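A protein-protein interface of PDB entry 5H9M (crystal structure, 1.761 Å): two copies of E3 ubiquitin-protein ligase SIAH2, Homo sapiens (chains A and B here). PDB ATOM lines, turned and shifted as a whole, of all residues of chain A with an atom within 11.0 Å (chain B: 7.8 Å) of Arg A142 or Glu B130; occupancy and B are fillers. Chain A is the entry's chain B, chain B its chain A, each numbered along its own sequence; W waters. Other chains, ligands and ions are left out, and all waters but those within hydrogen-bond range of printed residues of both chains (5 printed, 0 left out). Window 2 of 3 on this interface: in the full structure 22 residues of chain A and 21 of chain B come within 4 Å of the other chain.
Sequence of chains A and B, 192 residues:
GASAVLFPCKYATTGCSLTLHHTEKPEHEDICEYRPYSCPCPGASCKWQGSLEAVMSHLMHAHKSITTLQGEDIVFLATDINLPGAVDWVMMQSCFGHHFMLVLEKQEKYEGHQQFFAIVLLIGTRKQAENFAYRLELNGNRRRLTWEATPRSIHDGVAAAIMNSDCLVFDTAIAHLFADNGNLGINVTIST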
ATOM      1  N   GLU A 137      24.446   8.050   9.185  1.00  0.00           N
ATOM      2  CA  GLU A 137      24.502   6.597   9.278  1.00  0.00           C
ATOM      3  C   GLU A 137      23.419   5.996   8.404  1.00  0.00           C
ATOM      4  O   GLU A 137      22.253   6.371   8.534  1.00  0.00           O
ATOM      5  CB  GLU A 137      24.295   6.207  10.741  1.00  0.00           C
ATOM      6  CG  GLU A 137      24.573   4.772  11.098  1.00  0.00           C
ATOM      7  CD  GLU A 137      24.396   4.526  12.597  1.00  0.00           C
ATOM      8  OE1 GLU A 137      25.267   4.931  13.395  1.00  0.00           O
ATOM      9  OE2 GLU A 137      23.404   3.877  12.970  1.00  0.00           O
ATOM     10  N   LEU A 138      23.816   5.128   7.480  1.00  0.00           N
ATOM     11  CA  LEU A 138      22.897   4.272   6.733  1.00  0.00           C
ATOM     12  C   LEU A 138      22.913   2.947   7.490  1.00  0.00           C
ATOM     13  O   LEU A 138      23.977   2.359   7.663  1.00  0.00           O
ATOM     14  CB  LEU A 138      23.380   4.048   5.312  1.00  0.00           C
ATOM     15  CG  LEU A 138      23.639   5.217   4.359  1.00  0.00           C
ATOM     16  CD1 LEU A 138      23.888   4.699   2.955  1.00  0.00           C
ATOM     17  CD2 LEU A 138      22.502   6.198   4.332  1.00  0.00           C
ATOM     18  N   ASN A 139      21.750   2.509   7.951  1.00  0.00           N
ATOM     19  CA  ASN A 139      21.564   1.256   8.693  1.00  0.00           C
ATOM     20  C   ASN A 139      20.746   0.283   7.906  1.00  0.00           C
ATOM     21  O   ASN A 139      19.726   0.652   7.348  1.00  0.00           O
ATOM     22  CB  ASN A 139      20.784   1.519   9.958  1.00  0.00           C
ATOM     23  CG  ASN A 139      21.656   1.994  11.039  1.00  0.00           C
ATOM     24  OD1 ASN A 139      22.460   1.222  11.561  1.00  0.00           O
ATOM     25  ND2 ASN A 139      21.529   3.267  11.395  1.00  0.00           N
ATOM     26  N   GLY A 140      21.177  -0.965   7.865  1.00  0.00           N
ATOM     27  CA  GLY A 140      20.542  -1.941   6.991  1.00  0.00           C
ATOM     28  C   GLY A 140      20.608  -3.339   7.521  1.00  0.00           C
ATOM     29  O   GLY A 140      20.893  -3.547   8.698  1.00  0.00           O
ATOM     30  N   ASN A 141      20.294  -4.287   6.643  1.00  0.00           N
ATOM     31  CA  ASN A 141      20.373  -5.699   6.954  1.00  0.00           C
ATOM     32  C   ASN A 141      21.831  -6.071   7.194  1.00  0.00           C
ATOM     33  O   ASN A 141      22.556  -6.366   6.251  1.00  0.00           O
ATOM     34  CB  ASN A 141      19.774  -6.547   5.826  1.00  0.00           C
ATOM     35  CG  ASN A 141      19.764  -8.035   6.153  1.00  0.00           C
ATOM     36  OD1 ASN A 141      19.452  -8.438   7.279  1.00  0.00           O
ATOM     37  ND2 ASN A 141      20.105  -8.858   5.172  1.00  0.00           N
ATOM     38  N   ARG A 142      22.235  -6.004   8.461  1.00  0.00           N
ATOM     39  CA  ARG A 142      23.555  -6.426   8.920  1.00  0.00           C
ATOM     40  C   ARG A 142      24.704  -5.681   8.234  1.00  0.00           C
ATOM     41  O   ARG A 142      25.792  -6.229   8.002  1.00  0.00           O
ATOM     42  CB  ARG A 142      23.684  -7.947   8.783  1.00  0.00           C
ATOM     43  CG  ARG A 142      22.580  -8.659   9.567  1.00  0.00           C
ATOM     44  CD  ARG A 142      22.551 -10.141   9.306  1.00  0.00           C
ATOM     45  NE  ARG A 142      23.596 -10.870  10.021  1.00  0.00           N
ATOM     46  CZ  ARG A 142      23.552 -11.241  11.303  1.00  0.00           C
ATOM     47  NH1 ARG A 142      24.576 -11.931  11.806  1.00  0.00           N
ATOM     48  NH2 ARG A 142      22.518 -10.917  12.082  1.00  0.00           N
ATOM     49  N   ARG A 143      24.419  -4.426   7.888  1.00  0.00           N
ATOM     50  CA  ARG A 143      25.385  -3.515   7.297  1.00  0.00           C
ATOM     51  C   ARG A 143      25.166  -2.116   7.874  1.00  0.00           C
ATOM     52  O   ARG A 143      24.036  -1.739   8.226  1.00  0.00           O
ATOM     53  CB  ARG A 143      25.201  -3.426   5.801  1.00  0.00           C
ATOM     54  CG  ARG A 143      25.420  -4.708   5.034  1.00  0.00           C
ATOM     55  CD  ARG A 143      24.921  -4.561   3.612  1.00  0.00           C
ATOM     56  NE  ARG A 143      25.181  -5.773   2.845  1.00  0.00           N
ATOM     57  CZ  ARG A 143      24.389  -6.841   2.788  1.00  0.00           C
ATOM     58  NH1 ARG A 143      23.247  -6.914   3.478  1.00  0.00           N
ATOM     59  NH2 ARG A 143      24.752  -7.871   2.042  1.00  0.00           N
ATOM     60  N   ARG A 144      26.245  -1.347   7.945  1.00  0.00           N
ATOM     61  CA  ARG A 144      26.154   0.051   8.336  1.00  0.00           C
ATOM     62  C   ARG A 144      27.267   0.859   7.683  1.00  0.00           C
ATOM     63  O   ARG A 144      28.420   0.434   7.664  1.00  0.00           O
ATOM     64  CB  ARG A 144      26.220   0.197   9.842  1.00  0.00           C
ATOM     65  CG  ARG A 144      26.013   1.617  10.338  1.00  0.00           C
ATOM     66  CD  ARG A 144      26.134   1.680  11.852  1.00  0.00           C
ATOM     67  NE  ARG A 144      25.146   0.839  12.524  1.00  0.00           N
ATOM     68  CZ  ARG A 144      25.400   0.155  13.628  1.00  0.00           C
ATOM     69  NH1 ARG A 144      26.613   0.229  14.177  1.00  0.00           N
ATOM     70  NH2 ARG A 144      24.460  -0.594  14.188  1.00  0.00           N
ATOM     71  N   LEU A 145      26.906   2.035   7.174  1.00  0.00           N
ATOM     72  CA  LEU A 145      27.862   2.952   6.540  1.00  0.00           C
ATOM     73  C   LEU A 145      27.730   4.278   7.242  1.00  0.00           C
ATOM     74  O   LEU A 145      26.632   4.829   7.324  1.00  0.00           O
ATOM     75  CB  LEU A 145      27.571   3.091   5.048  1.00  0.00           C
ATOM     76  CG  LEU A 145      28.406   4.101   4.266  1.00  0.00           C
ATOM     77  CD1 LEU A 145      29.866   3.705   4.272  1.00  0.00           C
ATOM     78  CD2 LEU A 145      27.852   4.278   2.839  1.00  0.00           C
ATOM     79  N   LEU A 177      21.179  -1.300  -1.156  1.00  0.00           N
ATOM     80  CA  LEU A 177      21.393  -2.169   0.008  1.00  0.00           C
ATOM     81  C   LEU A 177      20.668  -1.649   1.242  1.00  0.00           C
ATOM     82  O   LEU A 177      20.319  -2.440   2.102  1.00  0.00           O
ATOM     83  CB  LEU A 177      22.876  -2.323   0.376  1.00  0.00           C
ATOM     84  CG  LEU A 177      23.824  -3.074  -0.577  1.00  0.00           C
ATOM     85  CD1 LEU A 177      25.273  -2.838  -0.176  1.00  0.00           C
ATOM     86  CD2 LEU A 177      23.482  -4.563  -0.621  1.00  0.00           C
ATOM     87  N   PHE A 178      20.508  -0.328   1.346  1.00  0.00           N
ATOM     88  CA  PHE A 178      19.941   0.312   2.534  1.00  0.00           C
ATOM     89  C   PHE A 178      18.511   0.788   2.345  1.00  0.00           C
ATOM     90  O   PHE A 178      17.824   1.108   3.323  1.00  0.00           O
ATOM     91  CB  PHE A 178      20.838   1.477   2.961  1.00  0.00           C
ATOM     92  CG  PHE A 178      22.166   1.028   3.508  1.00  0.00           C
ATOM     93  CD1 PHE A 178      22.231   0.403   4.736  1.00  0.00           C
ATOM     94  CD2 PHE A 178      23.327   1.193   2.789  1.00  0.00           C
ATOM     95  CE1 PHE A 178      23.447  -0.039   5.244  1.00  0.00           C
ATOM     96  CE2 PHE A 178      24.553   0.766   3.288  1.00  0.00           C
ATOM     97  CZ  PHE A 178      24.609   0.133   4.516  1.00  0.00           C
ATOM     98  N   ALA A 179      18.056   0.832   1.105  1.00  0.00           N
ATOM     99  CA  ALA A 179      16.735   1.375   0.799  1.00  0.00           C
ATOM    100  C   ALA A 179      15.622   0.440   1.211  1.00  0.00           C
ATOM    101  O   ALA A 179      15.790  -0.776   1.257  1.00  0.00           O
ATOM    102  CB  ALA A 179      16.622   1.664  -0.696  1.00  0.00           C
ATOM    103  N   GLU B  27      22.966 -24.859   2.985  1.00  0.00           N
ATOM    104  CA  GLU B  27      23.535 -24.816   4.338  1.00  0.00           C
ATOM    105  C   GLU B  27      24.599 -25.901   4.544  1.00  0.00           C
ATOM    106  O   GLU B  27      25.684 -25.627   5.085  1.00  0.00           O
ATOM    107  CB  GLU B  27      22.410 -24.983   5.368  1.00  0.00           C
ATOM    108  CG  GLU B  27      22.803 -24.758   6.822  1.00  0.00           C
ATOM    109  CD  GLU B  27      21.613 -24.811   7.777  1.00  0.00           C
ATOM    110  OE1 GLU B  27      20.479 -25.098   7.322  1.00  0.00           O
ATOM    111  OE2 GLU B  27      21.817 -24.570   8.989  1.00  0.00           O
ATOM    112  N   ASP B  30      27.797 -25.214   2.300  1.00  0.00           N
ATOM    113  CA  ASP B  30      28.620 -24.184   2.971  1.00  0.00           C
ATOM    114  C   ASP B  30      29.695 -24.814   3.878  1.00  0.00           C
ATOM    115  O   ASP B  30      30.868 -24.405   3.856  1.00  0.00           O
ATOM    116  CB  ASP B  30      27.716 -23.261   3.798  1.00  0.00           C
ATOM    117  CG  ASP B  30      28.491 -22.188   4.573  1.00  0.00           C
ATOM    118  OD1 ASP B  30      29.471 -21.630   4.032  1.00  0.00           O
ATOM    119  OD2 ASP B  30      28.090 -21.890   5.714  1.00  0.00           O
ATOM    120  N   LEU B 122      36.541 -14.193   5.986  1.00  0.00           N
ATOM    121  CA  LEU B 122      36.980 -15.191   6.922  1.00  0.00           C
ATOM    122  C   LEU B 122      37.548 -16.389   6.168  1.00  0.00           C
ATOM    123  O   LEU B 122      36.945 -16.869   5.218  1.00  0.00           O
ATOM    124  CB  LEU B 122      35.796 -15.631   7.801  1.00  0.00           C
ATOM    125  CG  LEU B 122      36.100 -16.812   8.709  1.00  0.00           C
ATOM    126  CD1 LEU B 122      37.115 -16.480   9.780  1.00  0.00           C
ATOM    127  CD2 LEU B 122      34.810 -17.347   9.310  1.00  0.00           C
ATOM    128  N   THR B 125      33.749 -20.776   6.797  1.00  0.00           N
ATOM    129  CA  THR B 125      32.483 -20.947   6.110  1.00  0.00           C
ATOM    130  C   THR B 125      31.608 -19.736   6.363  1.00  0.00           C
ATOM    131  O   THR B 125      31.907 -18.907   7.246  1.00  0.00           O
ATOM    132  CB  THR B 125      31.788 -22.199   6.656  1.00  0.00           C
ATOM    133  OG1 THR B 125      31.531 -22.006   8.042  1.00  0.00           O
ATOM    134  CG2 THR B 125      32.667 -23.442   6.489  1.00  0.00           C
ATOM    135  N   ARG B 126      30.521 -19.613   5.607  1.00  0.00           N
ATOM    136  CA  ARG B 126      29.533 -18.569   5.895  1.00  0.00           C
ATOM    137  C   ARG B 126      28.943 -18.720   7.295  1.00  0.00           C
ATOM    138  O   ARG B 126      28.725 -17.743   7.984  1.00  0.00           O
ATOM    139  CB  ARG B 126      28.395 -18.567   4.881  1.00  0.00           C
ATOM    140  CG  ARG B 126      28.685 -17.822   3.600  1.00  0.00           C
ATOM    141  CD  ARG B 126      27.355 -17.402   2.968  1.00  0.00           C
ATOM    142  NE  ARG B 126      26.495 -18.567   2.807  1.00  0.00           N
ATOM    143  CZ  ARG B 126      26.654 -19.512   1.880  1.00  0.00           C
ATOM    144  NH1 ARG B 126      27.633 -19.441   0.972  1.00  0.00           N
ATOM    145  NH2 ARG B 126      25.808 -20.541   1.849  1.00  0.00           N
ATOM    146  N   LYS B 127      28.706 -19.951   7.714  1.00  0.00           N
ATOM    147  CA  LYS B 127      28.145 -20.175   9.038  1.00  0.00           C
ATOM    148  C   LYS B 127      29.079 -19.646  10.122  1.00  0.00           C
ATOM    149  O   LYS B 127      28.626 -18.990  11.056  1.00  0.00           O
ATOM    150  CB  LYS B 127      27.803 -21.654   9.256  1.00  0.00           C
ATOM    151  CG  LYS B 127      27.040 -21.926  10.564  1.00  0.00           C
ATOM    152  CD  LYS B 127      25.763 -21.097  10.728  1.00  0.00           C
ATOM    153  CE  LYS B 127      24.924 -21.553  11.935  1.00  0.00           C
ATOM    154  NZ  LYS B 127      23.516 -21.073  11.843  1.00  0.00           N
ATOM    155  N   GLN B 128      30.373 -19.911   9.996  1.00  0.00           N
ATOM    156  CA  GLN B 128      31.371 -19.349  10.918  1.00  0.00           C
ATOM    157  C   GLN B 128      31.440 -17.835  10.803  1.00  0.00           C
ATOM    158  O   GLN B 128      31.462 -17.135  11.813  1.00  0.00           O
ATOM    159  CB  GLN B 128      32.753 -19.947  10.679  1.00  0.00           C
ATOM    160  CG  GLN B 128      32.855 -21.423  10.998  1.00  0.00           C
ATOM    161  CD  GLN B 128      34.142 -22.072  10.505  1.00  0.00           C
ATOM    162  OE1 GLN B 128      34.708 -21.701   9.473  1.00  0.00           O
ATOM    163  NE2 GLN B 128      34.608 -23.059  11.254  1.00  0.00           N
ATOM    164  N   ALA B 129      31.436 -17.334   9.574  1.00  0.00           N
ATOM    165  CA  ALA B 129      31.535 -15.882   9.329  1.00  0.00           C
ATOM    166  C   ALA B 129      30.412 -15.086   9.982  1.00  0.00           C
ATOM    167  O   ALA B 129      30.640 -13.977  10.453  1.00  0.00           O
ATOM    168  CB  ALA B 129      31.617 -15.584   7.839  1.00  0.00           C
ATOM    169  N   GLU B 130      29.214 -15.676  10.050  1.00  0.00           N
ATOM    170  CA  GLU B 130      28.062 -15.055  10.727  1.00  0.00           C
ATOM    171  C   GLU B 130      28.228 -14.805  12.236  1.00  0.00           C
ATOM    172  O   GLU B 130      27.491 -13.996  12.815  1.00  0.00           O
ATOM    173  CB  GLU B 130      26.789 -15.862  10.404  1.00  0.00           C
ATOM    174  CG  GLU B 130      26.347 -15.631   8.960  1.00  0.00           C
ATOM    175  CD  GLU B 130      25.438 -16.702   8.345  1.00  0.00           C
ATOM    176  OE1 GLU B 130      25.075 -17.695   9.025  1.00  0.00           O
ATOM    177  OE2 GLU B 130      25.091 -16.549   7.139  1.00  0.00           O
ATOM    178  N   ASN B 131      29.218 -15.434  12.870  1.00  0.00           N
ATOM    179  CA  ASN B 131      29.550 -15.161  14.280  1.00  0.00           C
ATOM    180  C   ASN B 131      30.282 -13.846  14.522  1.00  0.00           C
ATOM    181  O   ASN B 131      30.426 -13.451  15.666  1.00  0.00           O
ATOM    182  CB  ASN B 131      30.424 -16.285  14.840  1.00  0.00           C
ATOM    183  CG  ASN B 131      29.781 -17.642  14.698  1.00  0.00           C
ATOM    184  OD1 ASN B 131      28.560 -17.745  14.579  1.00  0.00           O
ATOM    185  ND2 ASN B 131      30.600 -18.689  14.658  1.00  0.00           N
ATOM    186  N   PHE B 132      30.731 -13.180  13.451  1.00  0.00           N
ATOM    187  CA  PHE B 132      31.560 -11.997  13.545  1.00  0.00           C
ATOM    188  C   PHE B 132      30.988 -10.798  12.825  1.00  0.00           C
ATOM    189  O   PHE B 132      30.240 -10.926  11.886  1.00  0.00           O
ATOM    190  CB  PHE B 132      32.922 -12.295  12.911  1.00  0.00           C
ATOM    191  CG  PHE B 132      33.634 -13.412  13.576  1.00  0.00           C
ATOM    192  CD1 PHE B 132      34.307 -13.184  14.765  1.00  0.00           C
ATOM    193  CD2 PHE B 132      33.576 -14.705  13.061  1.00  0.00           C
ATOM    194  CE1 PHE B 132      34.957 -14.222  15.425  1.00  0.00           C
ATOM    195  CE2 PHE B 132      34.232 -15.753  13.711  1.00  0.00           C
ATOM    196  CZ  PHE B 132      34.894 -15.506  14.908  1.00  0.00           C
ATOM    197  N   ALA B 133      31.420  -9.628  13.265  1.00  0.00           N
ATOM    198  CA  ALA B 133      31.220  -8.381  12.529  1.00  0.00           C
ATOM    199  C   ALA B 133      32.602  -7.848  12.296  1.00  0.00           C
ATOM    200  O   ALA B 133      33.488  -8.040  13.127  1.00  0.00           O
ATOM    201  CB  ALA B 133      30.412  -7.366  13.334  1.00  0.00           C
ATOM    202  N   TYR B 134      32.791  -7.136  11.189  1.00  0.00           N
ATOM    203  CA  TYR B 134      34.011  -6.373  11.004  1.00  0.00           C
ATOM    204  C   TYR B 134      33.678  -4.916  10.780  1.00  0.00           C
ATOM    205  O   TYR B 134      32.600  -4.591  10.284  1.00  0.00           O
ATOM    206  CB  TYR B 134      34.852  -6.910   9.856  1.00  0.00           C
ATOM    207  CG  TYR B 134      34.363  -6.633   8.453  1.00  0.00           C
ATOM    208  CD1 TYR B 134      33.444  -7.480   7.829  1.00  0.00           C
ATOM    209  CD2 TYR B 134      34.841  -5.545   7.734  1.00  0.00           C
ATOM    210  CE1 TYR B 134      33.015  -7.251   6.535  1.00  0.00           C
ATOM    211  CE2 TYR B 134      34.404  -5.292   6.448  1.00  0.00           C
ATOM    212  CZ  TYR B 134      33.500  -6.154   5.851  1.00  0.00           C
ATOM    213  OH  TYR B 134      33.117  -5.915   4.560  1.00  0.00           O
ATOM    214  N   TRP B 147      32.678   1.467   7.532  1.00  0.00           N
ATOM    215  CA  TRP B 147      31.830   0.396   6.993  1.00  0.00           C
ATOM    216  C   TRP B 147      31.838  -0.749   7.977  1.00  0.00           C
ATOM    217  O   TRP B 147      32.908  -1.141   8.440  1.00  0.00           O
ATOM    218  CB  TRP B 147      32.381  -0.099   5.652  1.00  0.00           C
ATOM    219  CG  TRP B 147      31.692  -1.290   5.091  1.00  0.00           C
ATOM    220  CD1 TRP B 147      32.142  -2.576   5.103  1.00  0.00           C
ATOM    221  CD2 TRP B 147      30.417  -1.329   4.458  1.00  0.00           C
ATOM    222  NE1 TRP B 147      31.250  -3.388   4.494  1.00  0.00           N
ATOM    223  CE2 TRP B 147      30.178  -2.659   4.085  1.00  0.00           C
ATOM    224  CE3 TRP B 147      29.464  -0.363   4.138  1.00  0.00           C
ATOM    225  CZ2 TRP B 147      29.002  -3.061   3.437  1.00  0.00           C
ATOM    226  CZ3 TRP B 147      28.291  -0.762   3.489  1.00  0.00           C
ATOM    227  CH2 TRP B 147      28.092  -2.102   3.132  1.00  0.00           C
ATOM    228  N   GLU B 148      30.659  -1.287   8.283  1.00  0.00           N
ATOM    229  CA  GLU B 148      30.534  -2.461   9.135  1.00  0.00           C
ATOM    230  C   GLU B 148      29.611  -3.476   8.489  1.00  0.00           C
ATOM    231  O   GLU B 148      28.566  -3.110   7.967  1.00  0.00           O
ATOM    232  CB  GLU B 148      29.980  -2.069  10.498  1.00  0.00           C
ATOM    233  CG  GLU B 148      30.817  -1.074  11.264  1.00  0.00           C
ATOM    234  CD  GLU B 148      30.080  -0.510  12.457  1.00  0.00           C
ATOM    235  OE1 GLU B 148      29.357   0.526  12.307  1.00  0.00           O
ATOM    236  OE2 GLU B 148      30.237  -1.116  13.552  1.00  0.00           O
ATOM    237  N   ALA B 149      29.993  -4.744   8.554  1.00  0.00           N
ATOM    238  CA  ALA B 149      29.255  -5.828   7.926  1.00  0.00           C
ATOM    239  C   ALA B 149      29.727  -7.181   8.502  1.00  0.00           C
ATOM    240  O   ALA B 149      30.599  -7.243   9.373  1.00  0.00           O
ATOM    241  CB  ALA B 149      29.448  -5.803   6.415  1.00  0.00           C
ATOM    242  N   THR B 150      29.104  -8.246   8.020  1.00  0.00           N
ATOM    243  CA  THR B 150      29.554  -9.608   8.287  1.00  0.00           C
ATOM    244  C   THR B 150      30.711  -9.975   7.332  1.00  0.00           C
ATOM    245  O   THR B 150      30.600  -9.734   6.121  1.00  0.00           O
ATOM    246  CB  THR B 150      28.369 -10.574   8.067  1.00  0.00           C
ATOM    247  OG1 THR B 150      27.271 -10.184   8.926  1.00  0.00           O
ATOM    248  CG2 THR B 150      28.783 -12.006   8.378  1.00  0.00           C
ATOM    249  N   PRO B 151      31.817 -10.553   7.855  1.00  0.00           N
ATOM    250  CA  PRO B 151      32.847 -11.059   6.928  1.00  0.00           C
ATOM    251  C   PRO B 151      32.283 -12.041   5.909  1.00  0.00           C
ATOM    252  O   PRO B 151      31.394 -12.845   6.233  1.00  0.00           O
ATOM    253  CB  PRO B 151      33.850 -11.773   7.843  1.00  0.00           C
ATOM    254  CG  PRO B 151      33.557 -11.356   9.216  1.00  0.00           C
ATOM    255  CD  PRO B 151      32.146 -10.844   9.255  1.00  0.00           C
ATOM    256  N   ARG B 152      32.778 -11.952   4.680  1.00  0.00           N
ATOM    257  CA  ARG B 152      32.436 -12.913   3.656  1.00  0.00           C
ATOM    258  C   ARG B 152      33.235 -14.160   3.863  1.00  0.00           C
ATOM    259  O   ARG B 152      34.391 -14.111   4.300  1.00  0.00           O
ATOM    260  CB  ARG B 152      32.738 -12.384   2.261  1.00  0.00           C
ATOM    261  CG  ARG B 152      31.713 -11.395   1.787  1.00  0.00           C
ATOM    262  CD  ARG B 152      32.165 -10.806   0.476  1.00  0.00           C
ATOM    263  NE  ARG B 152      31.940 -11.652  -0.684  1.00  0.00           N
ATOM    264  CZ  ARG B 152      30.756 -11.855  -1.265  1.00  0.00           C
ATOM    265  NH1 ARG B 152      29.637 -11.316  -0.771  1.00  0.00           N
ATOM    266  NH2 ARG B 152      30.691 -12.627  -2.349  1.00  0.00           N
ATOM    267  N   SER B 153      32.636 -15.297   3.554  1.00  0.00           N
ATOM    268  CA  SER B 153      33.404 -16.534   3.493  1.00  0.00           C
ATOM    269  C   SER B 153      34.357 -16.468   2.285  1.00  0.00           C
ATOM    270  O   SER B 153      33.964 -16.017   1.208  1.00  0.00           O
ATOM    271  CB  SER B 153      32.464 -17.725   3.288  1.00  0.00           C
ATOM    272  OG  SER B 153      33.223 -18.888   2.975  1.00  0.00           O
ATOM    273  N   ASP B 166      29.371  -4.227  -2.047  1.00  0.00           N
ATOM    274  CA  ASP B 166      28.974  -4.721  -0.712  1.00  0.00           C
ATOM    275  C   ASP B 166      30.233  -4.818   0.116  1.00  0.00           C
ATOM    276  O   ASP B 166      30.658  -5.900   0.502  1.00  0.00           O
ATOM    277  CB  ASP B 166      28.272  -6.083  -0.822  1.00  0.00           C
ATOM    278  CG  ASP B 166      27.615  -6.538   0.491  1.00  0.00           C
ATOM    279  OD1 ASP B 166      27.582  -5.782   1.495  1.00  0.00           O
ATOM    280  OD2 ASP B 166      27.100  -7.670   0.508  1.00  0.00           O
ATOM    281  N   SER B 191      34.752  -8.114  15.775  1.00  0.00           N
ATOM    282  CA  SER B 191      34.048  -8.316  17.021  1.00  0.00           C
ATOM    283  C   SER B 191      33.181  -9.550  16.935  1.00  0.00           C
ATOM    284  O   SER B 191      32.827 -10.012  15.855  1.00  0.00           O
ATOM    285  CB  SER B 191      33.214  -7.100  17.372  1.00  0.00           C
ATOM    286  OG  SER B 191      32.358  -6.764  16.314  1.00  0.00           O
ATOM    287  N   THR B 192      32.877 -10.097  18.107  1.00  0.00           N
ATOM    288  CA  THR B 192      32.050 -11.285  18.191  1.00  0.00           C
ATOM    289  C   THR B 192      31.237 -11.259  19.463  1.00  0.00           C
ATOM    290  O   THR B 192      30.256 -11.987  19.590  1.00  0.00           O
ATOM    291  CB  THR B 192      32.898 -12.562  18.113  1.00  0.00           C
ATOM    292  OG1 THR B 192      32.041 -13.686  17.929  1.00  0.00           O
ATOM    293  CG2 THR B 192      33.786 -12.750  19.379  1.00  0.00           C
ATOM    294  OXT THR B 192      31.561 -10.515  20.386  1.00  0.00           O
HETATM  295  O   HOH W   1      29.026   2.100  14.448  1.00  0.00           O
HETATM  296  O   HOH W   2      26.674  -8.040   6.050  1.00  0.00           O
HETATM  297  O   HOH W   3      25.134 -11.585   8.028  1.00  0.00           O
HETATM  298  O   HOH W   4      27.412 -11.395  11.383  1.00  0.00           O
HETATM  299  O   HOH W   5      29.535   2.054  10.091  1.00  0.00           O
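NH1 of Arg A142 touches O of Glu B130 (3.7 Å).
O of Arg A142 touches CA of Ala B149, 3.5 Å away.
O of Arg A142 touches N of Thr B150, 3.9 Å away.
CA of Arg A143 touches O of Glu B148, 3.3 Å away.
CA of Trp B147 touches O of Arg A144, at 3.5 Å.
Phe A178 touches Trp B147.
Water W3 bridges the guanidinium group (NE) of Arg A142 and the side-chain hydroxyl (OG1) of Thr B150.
Water W1 bridges OE1 of Glu B148 (2.7 Å) and NH1 of Arg A144 (3.1 Å).
Water W5 bridges OE1 of Glu B148 (2.7 Å) and O of Arg A144 (3.1 Å).
Water W4 lies within hydrogen-bond range of OG1 of Thr B150 (2.7 Å), O of Phe B132 (2.9 Å), NH1 of Arg A142 (2.9 Å) and O of Glu B130 (3.0 Å).
Water W2 bridges O of Arg A142 (2.8 Å) and N of Thr B150 (3.1 Å).
OD1 of Asp B166 lies within salt-bridge range of NE of Arg A143.
NH1 of Arg A144 is in salt-bridge range of OE1 of Glu B148.
Glu A137 touches none of the printed residues of chain B.
Of the printed residues of chain B, Arg A142 touches Glu B130 (3.7 Å), Ala B149 (3.5 Å) and Thr B150 (3.9 Å).
Printed residues of chain B within 4 Å of Arg A143: Glu B148 (3.3 Å) and Asp B166 (2.8 Å).
Of the printed residues of chain B, Arg A144 touches Trp B147 and Glu B148.
Of the printed residues of chain B, Phe A178 touches Trp B147.
No residue of chain A comes within 4 Å of Ala B129.
No residue of chain A comes within 4 Å of Asn B131.
Of the printed residues of chain A, Trp B147 touches Arg A144 (3.5 Å) and Phe A178 (3.9 Å).
Of the printed residues of chain A, Glu B148 touches Arg A143 and Arg A144.
The nearest residue of chain A that does not touch Glu B130 is Asn A141 (9.4 Å).
The nearest printed residue of chain A that does not touch Asp B166 is Leu A177 (4.1 Å).
The backbone carbonyl oxygen (O) of Asn A141 is in hydrogen-bond range of the guanidinium group (NH1) of Arg A143 (2.9 Å).
OH of Tyr B134 is in hydrogen-bond range of NE1 of Trp B147 (3.1 Å).
OD1 of Asn A139 sits at hydrogen-bond distance from NE of Arg A144 (2.9 Å).
The side-chain carboxylate (OE2) of Glu A137 is in salt-bridge range of the guanidinium group (NE) of Arg A144 (3.5 Å).
The backbone carbonyl oxygen (O) of Ala B149 is in hydrogen-bond range of the backbone NH (N) of Tyr B134, at 2.8 Å.
No position is printed for both chains.
Of the 8 pairs that touch across the chains among the printed residues, none has its exchanged pair printed and touching as well.
Hydrophobic or aromatic side chains of chain A that line the printed part of chain B: Phe A178.
Among the printed residues, 8 pairs touch across the chains.
Among the printed residues, Asp or Glu carboxylates within 4 Å of a Lys or Arg side-chain nitrogen of the other chain: Arg A143 with Asp B166 (2.8 Å) and Arg A144 with Glu B148 (3.3 Å).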
